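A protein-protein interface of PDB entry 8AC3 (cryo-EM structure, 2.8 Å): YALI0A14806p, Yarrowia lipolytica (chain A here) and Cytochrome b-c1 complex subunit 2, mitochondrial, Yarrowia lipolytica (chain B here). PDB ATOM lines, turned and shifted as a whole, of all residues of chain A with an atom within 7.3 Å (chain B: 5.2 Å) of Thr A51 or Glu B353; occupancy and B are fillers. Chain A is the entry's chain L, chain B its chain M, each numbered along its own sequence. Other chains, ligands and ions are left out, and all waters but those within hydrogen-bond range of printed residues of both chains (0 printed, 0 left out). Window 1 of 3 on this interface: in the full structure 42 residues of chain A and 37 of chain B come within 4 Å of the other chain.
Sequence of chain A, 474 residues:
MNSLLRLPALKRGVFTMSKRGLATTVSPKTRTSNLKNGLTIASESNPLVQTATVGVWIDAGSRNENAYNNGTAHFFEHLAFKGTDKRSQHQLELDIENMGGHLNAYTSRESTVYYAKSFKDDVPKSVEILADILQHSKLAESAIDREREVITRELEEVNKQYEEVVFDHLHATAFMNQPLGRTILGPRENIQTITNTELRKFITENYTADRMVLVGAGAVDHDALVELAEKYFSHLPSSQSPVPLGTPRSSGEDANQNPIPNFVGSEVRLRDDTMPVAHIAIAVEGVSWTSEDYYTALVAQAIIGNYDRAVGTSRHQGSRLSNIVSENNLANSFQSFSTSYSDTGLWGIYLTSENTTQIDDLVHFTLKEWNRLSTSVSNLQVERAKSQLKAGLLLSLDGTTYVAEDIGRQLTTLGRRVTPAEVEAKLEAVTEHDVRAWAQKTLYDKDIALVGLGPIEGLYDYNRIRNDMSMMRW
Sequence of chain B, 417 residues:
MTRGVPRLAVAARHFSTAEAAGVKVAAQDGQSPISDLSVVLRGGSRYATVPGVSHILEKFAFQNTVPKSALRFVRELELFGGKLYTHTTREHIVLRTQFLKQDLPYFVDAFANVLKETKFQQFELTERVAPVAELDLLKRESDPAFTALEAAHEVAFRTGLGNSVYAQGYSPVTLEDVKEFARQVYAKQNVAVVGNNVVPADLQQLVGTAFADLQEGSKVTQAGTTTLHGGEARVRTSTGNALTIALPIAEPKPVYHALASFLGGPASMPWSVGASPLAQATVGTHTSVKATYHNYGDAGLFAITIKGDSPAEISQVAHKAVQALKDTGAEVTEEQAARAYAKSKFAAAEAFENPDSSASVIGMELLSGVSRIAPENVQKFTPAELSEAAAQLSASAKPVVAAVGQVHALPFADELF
O of Gln A50 sits at hydrogen-bond distance from N of Lys A120 (3.2 Å).
The side-chain hydroxyl (OG1) of Thr A51 sits at hydrogen-bond distance from the backbone carbonyl oxygen (O) of Ser A118, 3.0 Å away.
The backbone carbonyl oxygen of Thr A51 is in hydrogen-bond range of the backbone NH of Ala A219 (3.2 Å).
The backbone carbonyl oxygen of Ala A52 lies within hydrogen-bond range of the backbone NH of Ser A118 (2.9 Å).
The side-chain amino group of Lys A117 is in hydrogen-bond range of the side-chain hydroxyl of Thr A400, 2.9 Å away.
Of the printed residues of chain B, Val A49 touches Glu B353.
Thr A51 touches just these residues of chain B: Phe B346, Ala B349 and Glu B353.
Of the printed residues of chain B, Lys A117 touches Phe B346 (3.99 Å).
Printed residues of chain B within 4 Å of Phe A119: Ala B349 (3.4 Å).
Of the printed residues of chain A, Phe B346 touches Thr A51, Lys A117 and Ser A118.
Printed residues of chain A within 4 Å of Ala B349: Thr A51 and Phe A119.
Glu B353 touches just these residues of chain A: Val A49 (3.8 Å), Gln A50 (3.6 Å) and Thr A51 (3.2 Å).
The nearest residue of chain A that does not touch Glu B353 is Lys A117 (4.5 Å).
The nearest printed residue of chain B that does not touch Val A49 is Phe B352 (6.7 Å).
Val A49 touches Glu B353 (CG1 to CG, 3.8 Å).
N of Gln A50 touches OE2 of Glu B353, at 3.6 Å.
Thr A51 touches Phe B346 (OG1 to CE1, 3.8 Å).
Thr A51 touches Ala B349.
OE1 of Glu B353 touches CB of Thr A51, at 3.2 Å.
Lys A117 touches Phe B346.
Phe B346 touches Ser A118.
CE1 of Phe A119 touches CB of Ala B349 (3.4 Å).
Of the 20 printed residues of chain A, 6 touch a printed residue of chain B.
Printed residues of chain A that touch a printed residue of chain B: Val A49, Gln A50, Thr A51, Lys A117, Ser A118 and Phe A119.
Hydrophobic or aromatic side chains of chain A that line the printed part of chain B: Val A49 and Phe A119.
Hydrophobic or aromatic side chains of chain B that line the printed part of chain A: Phe B346 and Ala B349.
Along chain B the printed residues that touch a printed residue of chain A span positions 346 to 353.
Among the printed residues, 8 pairs touch across the chains.
Among the printed residues, no Asp or Glu carboxylate lies within 4 Å of a Lys or Arg side-chain nitrogen of the other chain.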
ATOM      1  N   ASN A  46      10.314 -19.072  -8.981  1.00  0.00           N
ATOM      2  CA  ASN A  46       9.423 -18.054  -9.512  1.00  0.00           C
ATOM      3  C   ASN A  46      10.023 -17.512 -10.808  1.00  0.00           C
ATOM      4  O   ASN A  46      10.870 -16.623 -10.770  1.00  0.00           O
ATOM      5  CB  ASN A  46       9.172 -16.939  -8.493  1.00  0.00           C
ATOM      6  CG  ASN A  46       8.116 -15.944  -8.925  1.00  0.00           C
ATOM      7  OD1 ASN A  46       7.358 -16.181  -9.865  1.00  0.00           O
ATOM      8  ND2 ASN A  46       8.027 -14.837  -8.209  1.00  0.00           N
ATOM      9  N   LEU A  48       9.296 -15.485 -12.925  1.00  0.00           N
ATOM     10  CA  LEU A  48       8.874 -14.125 -13.219  1.00  0.00           C
ATOM     11  C   LEU A  48       9.887 -13.111 -12.690  1.00  0.00           C
ATOM     12  O   LEU A  48       9.885 -11.960 -13.124  1.00  0.00           O
ATOM     13  CB  LEU A  48       7.498 -13.877 -12.592  1.00  0.00           C
ATOM     14  CG  LEU A  48       6.305 -13.817 -13.548  1.00  0.00           C
ATOM     15  CD1 LEU A  48       5.316 -12.757 -13.091  1.00  0.00           C
ATOM     16  CD2 LEU A  48       6.728 -13.565 -14.991  1.00  0.00           C
ATOM     17  N   VAL A  49      10.724 -13.529 -11.731  1.00  0.00           N
ATOM     18  CA  VAL A  49      11.730 -12.650 -11.150  1.00  0.00           C
ATOM     19  C   VAL A  49      13.106 -13.035 -11.681  1.00  0.00           C
ATOM     20  O   VAL A  49      13.279 -14.088 -12.292  1.00  0.00           O
ATOM     21  CB  VAL A  49      11.704 -12.625  -9.606  1.00  0.00           C
ATOM     22  CG1 VAL A  49      10.433 -11.998  -9.055  1.00  0.00           C
ATOM     23  CG2 VAL A  49      11.983 -13.989  -8.984  1.00  0.00           C
ATOM     24  N   GLN A  50      14.083 -12.170 -11.395  1.00  0.00           N
ATOM     25  CA  GLN A  50      15.426 -12.290 -11.932  1.00  0.00           C
ATOM     26  C   GLN A  50      16.447 -12.395 -10.803  1.00  0.00           C
ATOM     27  O   GLN A  50      17.635 -12.576 -11.053  1.00  0.00           O
ATOM     28  CB  GLN A  50      15.708 -11.108 -12.859  1.00  0.00           C
ATOM     29  CG  GLN A  50      15.386 -11.416 -14.316  1.00  0.00           C
ATOM     30  CD  GLN A  50      16.580 -11.254 -15.228  1.00  0.00           C
ATOM     31  OE1 GLN A  50      17.025 -10.143 -15.510  1.00  0.00           O
ATOM     32  NE2 GLN A  50      17.099 -12.371 -15.718  1.00  0.00           N
ATOM     33  N   THR A  51      15.962 -12.292  -9.564  1.00  0.00           N
ATOM     34  CA  THR A  51      16.791 -12.308  -8.376  1.00  0.00           C
ATOM     35  C   THR A  51      16.460 -13.554  -7.563  1.00  0.00           C
ATOM     36  O   THR A  51      15.331 -14.029  -7.621  1.00  0.00           O
ATOM     37  CB  THR A  51      16.587 -10.975  -7.649  1.00  0.00           C
ATOM     38  OG1 THR A  51      17.709 -10.182  -8.035  1.00  0.00           O
ATOM     39  CG2 THR A  51      16.416 -11.084  -6.153  1.00  0.00           C
ATOM     40  N   ALA A  52      17.423 -14.053  -6.776  1.00  0.00           N
ATOM     41  CA  ALA A  52      17.193 -15.201  -5.908  1.00  0.00           C
ATOM     42  C   ALA A  52      17.615 -14.898  -4.476  1.00  0.00           C
ATOM     43  O   ALA A  52      18.542 -14.130  -4.264  1.00  0.00           O
ATOM     44  CB  ALA A  52      17.940 -16.382  -6.448  1.00  0.00           C
ATOM     45  N   THR A  53      16.925 -15.494  -3.499  1.00  0.00           N
ATOM     46  CA  THR A  53      17.408 -15.505  -2.127  1.00  0.00           C
ATOM     47  C   THR A  53      17.762 -16.941  -1.748  1.00  0.00           C
ATOM     48  O   THR A  53      16.864 -17.759  -1.609  1.00  0.00           O
ATOM     49  CB  THR A  53      16.373 -14.889  -1.172  1.00  0.00           C
ATOM     50  OG1 THR A  53      16.142 -13.546  -1.596  1.00  0.00           O
ATOM     51  CG2 THR A  53      16.846 -14.861   0.262  1.00  0.00           C
ATOM     52  N   LYS A 117      21.032 -12.521  -0.989  1.00  0.00           N
ATOM     53  CA  LYS A 117      20.215 -12.096  -2.105  1.00  0.00           C
ATOM     54  C   LYS A 117      21.147 -11.783  -3.264  1.00  0.00           C
ATOM     55  O   LYS A 117      22.128 -11.075  -3.074  1.00  0.00           O
ATOM     56  CB  LYS A 117      19.385 -10.881  -1.704  1.00  0.00           C
ATOM     57  CG  LYS A 117      18.110 -10.738  -2.509  1.00  0.00           C
ATOM     58  CD  LYS A 117      17.209  -9.651  -1.954  1.00  0.00           C
ATOM     59  CE  LYS A 117      16.129  -9.164  -2.900  1.00  0.00           C
ATOM     60  NZ  LYS A 117      14.976 -10.095  -2.991  1.00  0.00           N
ATOM     61  N   SER A 118      20.854 -12.339  -4.440  1.00  0.00           N
ATOM     62  CA  SER A 118      21.757 -12.189  -5.563  1.00  0.00           C
ATOM     63  C   SER A 118      20.981 -12.128  -6.872  1.00  0.00           C
ATOM     64  O   SER A 118      19.754 -12.045  -6.895  1.00  0.00           O
ATOM     65  CB  SER A 118      22.793 -13.295  -5.588  1.00  0.00           C
ATOM     66  OG  SER A 118      22.170 -14.562  -5.749  1.00  0.00           O
ATOM     67  N   PHE A 119      21.748 -12.157  -7.959  1.00  0.00           N
ATOM     68  CA  PHE A 119      21.217 -12.322  -9.291  1.00  0.00           C
ATOM     69  C   PHE A 119      21.058 -13.811  -9.583  1.00  0.00           C
ATOM     70  O   PHE A 119      21.556 -14.638  -8.823  1.00  0.00           O
ATOM     71  CB  PHE A 119      22.107 -11.557 -10.269  1.00  0.00           C
ATOM     72  CG  PHE A 119      21.282 -10.962 -11.368  1.00  0.00           C
ATOM     73  CD1 PHE A 119      20.488  -9.851 -11.121  1.00  0.00           C
ATOM     74  CD2 PHE A 119      21.197 -11.590 -12.602  1.00  0.00           C
ATOM     75  CE1 PHE A 119      19.669  -9.344 -12.119  1.00  0.00           C
ATOM     76  CE2 PHE A 119      20.376 -11.081 -13.598  1.00  0.00           C
ATOM     77  CZ  PHE A 119      19.609  -9.963 -13.350  1.00  0.00           C
ATOM     78  N   LYS A 120      20.347 -14.146 -10.663  1.00  0.00           N
ATOM     79  CA  LYS A 120      19.961 -15.518 -10.962  1.00  0.00           C
ATOM     80  C   LYS A 120      21.187 -16.430 -11.069  1.00  0.00           C
ATOM     81  O   LYS A 120      21.184 -17.555 -10.566  1.00  0.00           O
ATOM     82  CB  LYS A 120      19.091 -15.539 -12.223  1.00  0.00           C
ATOM     83  CG  LYS A 120      18.772 -16.917 -12.792  1.00  0.00           C
ATOM     84  CD  LYS A 120      18.106 -16.850 -14.166  1.00  0.00           C
ATOM     85  CE  LYS A 120      17.830 -18.205 -14.795  1.00  0.00           C
ATOM     86  NZ  LYS A 120      17.176 -18.093 -16.125  1.00  0.00           N
ATOM     87  N   VAL A 123      24.064 -17.469  -8.016  1.00  0.00           N
ATOM     88  CA  VAL A 123      23.631 -18.301  -6.912  1.00  0.00           C
ATOM     89  C   VAL A 123      24.759 -19.248  -6.510  1.00  0.00           C
ATOM     90  O   VAL A 123      25.010 -19.406  -5.321  1.00  0.00           O
ATOM     91  CB  VAL A 123      22.302 -19.014  -7.218  1.00  0.00           C
ATOM     92  CG1 VAL A 123      22.096 -20.277  -6.395  1.00  0.00           C
ATOM     93  CG2 VAL A 123      21.137 -18.054  -7.053  1.00  0.00           C
ATOM     94  N   ALA A 217      14.647 -19.269  -2.896  1.00  0.00           N
ATOM     95  CA  ALA A 217      13.424 -18.710  -3.451  1.00  0.00           C
ATOM     96  C   ALA A 217      13.759 -17.732  -4.571  1.00  0.00           C
ATOM     97  O   ALA A 217      14.720 -16.975  -4.468  1.00  0.00           O
ATOM     98  CB  ALA A 217      12.622 -18.040  -2.367  1.00  0.00           C
ATOM     99  N   GLY A 218      12.907 -17.710  -5.601  1.00  0.00           N
ATOM    100  CA  GLY A 218      13.058 -16.813  -6.730  1.00  0.00           C
ATOM    101  C   GLY A 218      13.606 -17.568  -7.929  1.00  0.00           C
ATOM    102  O   GLY A 218      13.129 -18.656  -8.235  1.00  0.00           O
ATOM    103  N   ALA A 219      14.632 -17.011  -8.565  1.00  0.00           N
ATOM    104  CA  ALA A 219      15.155 -17.628  -9.768  1.00  0.00           C
ATOM    105  C   ALA A 219      16.202 -18.683  -9.410  1.00  0.00           C
ATOM    106  O   ALA A 219      17.397 -18.472  -9.604  1.00  0.00           O
ATOM    107  CB  ALA A 219      15.685 -16.557 -10.682  1.00  0.00           C
ATOM    108  N   VAL A 220      15.734 -19.816  -8.872  1.00  0.00           N
ATOM    109  CA  VAL A 220      16.597 -20.926  -8.497  1.00  0.00           C
ATOM    110  C   VAL A 220      16.028 -22.176  -9.148  1.00  0.00           C
ATOM    111  O   VAL A 220      14.815 -22.345  -9.180  1.00  0.00           O
ATOM    112  CB  VAL A 220      16.631 -21.133  -6.971  1.00  0.00           C
ATOM    113  CG1 VAL A 220      17.807 -21.995  -6.536  1.00  0.00           C
ATOM    114  CG2 VAL A 220      16.594 -19.829  -6.200  1.00  0.00           C
ATOM    115  N   ASP A 398       5.560 -11.359  -0.366  1.00  0.00           N
ATOM    116  CA  ASP A 398       5.708 -10.461  -1.499  1.00  0.00           C
ATOM    117  C   ASP A 398       6.915 -10.858  -2.363  1.00  0.00           C
ATOM    118  O   ASP A 398       6.757 -11.464  -3.426  1.00  0.00           O
ATOM    119  CB  ASP A 398       5.855  -9.020  -0.994  1.00  0.00           C
ATOM    120  CG  ASP A 398       4.686  -8.512  -0.162  1.00  0.00           C
ATOM    121  OD1 ASP A 398       3.580  -8.354  -0.722  1.00  0.00           O
ATOM    122  OD2 ASP A 398       4.881  -8.300   1.049  1.00  0.00           O
ATOM    123  N   GLY A 399       8.121 -10.491  -1.903  1.00  0.00           N
ATOM    124  CA  GLY A 399       9.366 -10.684  -2.631  1.00  0.00           C
ATOM    125  C   GLY A 399      10.059 -11.980  -2.218  1.00  0.00           C
ATOM    126  O   GLY A 399       9.568 -12.707  -1.354  1.00  0.00           O
ATOM    127  N   THR A 400      11.213 -12.245  -2.834  1.00  0.00           N
ATOM    128  CA  THR A 400      11.863 -13.536  -2.678  1.00  0.00           C
ATOM    129  C   THR A 400      12.344 -13.730  -1.244  1.00  0.00           C
ATOM    130  O   THR A 400      12.406 -14.864  -0.778  1.00  0.00           O
ATOM    131  CB  THR A 400      13.027 -13.725  -3.657  1.00  0.00           C
ATOM    132  OG1 THR A 400      14.061 -12.810  -3.304  1.00  0.00           O
ATOM    133  CG2 THR A 400      12.637 -13.540  -5.105  1.00  0.00           C
ATOM    134  N   THR A 401      12.709 -12.633  -0.569  1.00  0.00           N
ATOM    135  CA  THR A 401      13.213 -12.743   0.788  1.00  0.00           C
ATOM    136  C   THR A 401      12.083 -13.169   1.718  1.00  0.00           C
ATOM    137  O   THR A 401      12.319 -13.931   2.649  1.00  0.00           O
ATOM    138  CB  THR A 401      13.949 -11.477   1.248  1.00  0.00           C
ATOM    139  OG1 THR A 401      15.027 -11.349   0.329  1.00  0.00           O
ATOM    140  CG2 THR A 401      14.560 -11.590   2.630  1.00  0.00           C
ATOM    141  N   PHE B 346      22.015  -5.615 -10.304  1.00  0.00           N
ATOM    142  CA  PHE B 346      21.292  -6.095  -9.147  1.00  0.00           C
ATOM    143  C   PHE B 346      20.334  -5.017  -8.671  1.00  0.00           C
ATOM    144  O   PHE B 346      19.200  -5.327  -8.334  1.00  0.00           O
ATOM    145  CB  PHE B 346      22.234  -6.482  -8.007  1.00  0.00           C
ATOM    146  CG  PHE B 346      21.504  -6.959  -6.778  1.00  0.00           C
ATOM    147  CD1 PHE B 346      20.916  -8.217  -6.747  1.00  0.00           C
ATOM    148  CD2 PHE B 346      21.393  -6.151  -5.655  1.00  0.00           C
ATOM    149  CE1 PHE B 346      20.234  -8.658  -5.618  1.00  0.00           C
ATOM    150  CE2 PHE B 346      20.715  -6.592  -4.524  1.00  0.00           C
ATOM    151  CZ  PHE B 346      20.134  -7.844  -4.509  1.00  0.00           C
ATOM    152  N   ALA B 349      17.318  -4.939 -10.799  1.00  0.00           N
ATOM    153  CA  ALA B 349      16.465  -6.109 -10.660  1.00  0.00           C
ATOM    154  C   ALA B 349      15.562  -5.961  -9.442  1.00  0.00           C
ATOM    155  O   ALA B 349      14.356  -6.115  -9.565  1.00  0.00           O
ATOM    156  CB  ALA B 349      17.292  -7.367 -10.590  1.00  0.00           C
ATOM    157  N   GLU B 350      16.148  -5.624  -8.291  1.00  0.00           N
ATOM    158  CA  GLU B 350      15.412  -5.546  -7.038  1.00  0.00           C
ATOM    159  C   GLU B 350      14.407  -4.390  -7.059  1.00  0.00           C
ATOM    160  O   GLU B 350      13.390  -4.442  -6.358  1.00  0.00           O
ATOM    161  CB  GLU B 350      16.376  -5.526  -5.853  1.00  0.00           C
ATOM    162  CG  GLU B 350      17.156  -4.228  -5.748  1.00  0.00           C
ATOM    163  CD  GLU B 350      18.244  -4.132  -4.697  1.00  0.00           C
ATOM    164  OE1 GLU B 350      19.246  -3.434  -4.966  1.00  0.00           O
ATOM    165  OE2 GLU B 350      18.072  -4.724  -3.610  1.00  0.00           O
ATOM    166  N   ALA B 351      14.684  -3.362  -7.873  1.00  0.00           N
ATOM    167  CA  ALA B 351      13.767  -2.242  -8.016  1.00  0.00           C
ATOM    168  C   ALA B 351      12.519  -2.681  -8.781  1.00  0.00           C
ATOM    169  O   ALA B 351      11.401  -2.294  -8.450  1.00  0.00           O
ATOM    170  CB  ALA B 351      14.457  -1.077  -8.683  1.00  0.00           C
ATOM    171  N   PHE B 352      12.719  -3.513  -9.800  1.00  0.00           N
ATOM    172  CA  PHE B 352      11.627  -4.005 -10.618  1.00  0.00           C
ATOM    173  C   PHE B 352      10.839  -5.092  -9.877  1.00  0.00           C
ATOM    174  O   PHE B 352       9.760  -5.483 -10.318  1.00  0.00           O
ATOM    175  CB  PHE B 352      12.216  -4.442 -11.956  1.00  0.00           C
ATOM    176  CG  PHE B 352      11.218  -4.723 -13.041  1.00  0.00           C
ATOM    177  CD1 PHE B 352      10.307  -3.749 -13.420  1.00  0.00           C
ATOM    178  CD2 PHE B 352      11.198  -5.950 -13.693  1.00  0.00           C
ATOM    179  CE1 PHE B 352       9.382  -4.000 -14.423  1.00  0.00           C
ATOM    180  CE2 PHE B 352      10.267  -6.204 -14.689  1.00  0.00           C
ATOM    181  CZ  PHE B 352       9.357  -5.232 -15.049  1.00  0.00           C
ATOM    182  N   GLU B 353      11.368  -5.557  -8.734  1.00  0.00           N
ATOM    183  CA  GLU B 353      10.702  -6.583  -7.943  1.00  0.00           C
ATOM    184  C   GLU B 353       9.823  -5.949  -6.870  1.00  0.00           C
ATOM    185  O   GLU B 353       8.654  -6.318  -6.768  1.00  0.00           O
ATOM    186  CB  GLU B 353      11.694  -7.577  -7.343  1.00  0.00           C
ATOM    187  CG  GLU B 353      12.157  -8.635  -8.335  1.00  0.00           C
ATOM    188  CD  GLU B 353      13.656  -8.918  -8.327  1.00  0.00           C
ATOM    189  OE1 GLU B 353      14.270  -8.774  -7.250  1.00  0.00           O
ATOM    190  OE2 GLU B 353      14.232  -9.192  -9.416  1.00  0.00           O
ATOM    191  N   ASN B 354      10.382  -5.009  -6.086  1.00  0.00           N
ATOM    192  CA  ASN B 354       9.624  -4.289  -5.065  1.00  0.00           C
ATOM    193  C   ASN B 354       8.401  -3.630  -5.708  1.00  0.00           C
ATOM    194  O   ASN B 354       8.569  -2.810  -6.613  1.00  0.00           O
ATOM    195  CB  ASN B 354      10.479  -3.271  -4.301  1.00  0.00           C
ATOM    196  CG  ASN B 354       9.675  -2.291  -3.462  1.00  0.00           C
ATOM    197  OD1 ASN B 354       8.847  -2.653  -2.626  1.00  0.00           O
ATOM    198  ND2 ASN B 354       9.911  -1.018  -3.678  1.00  0.00           N
ATOM    199  N   PRO B 355       7.150  -3.954  -5.273  1.00  0.00           N
ATOM    200  CA  PRO B 355       5.939  -3.447  -5.925  1.00  0.00           C
ATOM    201  C   PRO B 355       5.833  -1.925  -5.968  1.00  0.00           C
ATOM    202  O   PRO B 355       5.310  -1.380  -6.936  1.00  0.00           O
ATOM    203  CB  PRO B 355       4.785  -4.009  -5.082  1.00  0.00           C
ATOM    204  CG  PRO B 355       5.418  -4.350  -3.762  1.00  0.00           C
ATOM    205  CD  PRO B 355       6.816  -4.813  -4.122  1.00  0.00           C
ATOM    206  N   SER B 358       8.308  -0.882  -8.692  1.00  0.00           N
ATOM    207  CA  SER B 358       7.900  -1.555  -9.918  1.00  0.00           C
ATOM    208  C   SER B 358       6.852  -0.726 -10.654  1.00  0.00           C
ATOM    209  O   SER B 358       7.011  -0.430 -11.839  1.00  0.00           O
ATOM    210  CB  SER B 358       7.395  -2.951  -9.642  1.00  0.00           C
ATOM    211  OG  SER B 358       7.096  -3.660 -10.828  1.00  0.00           O
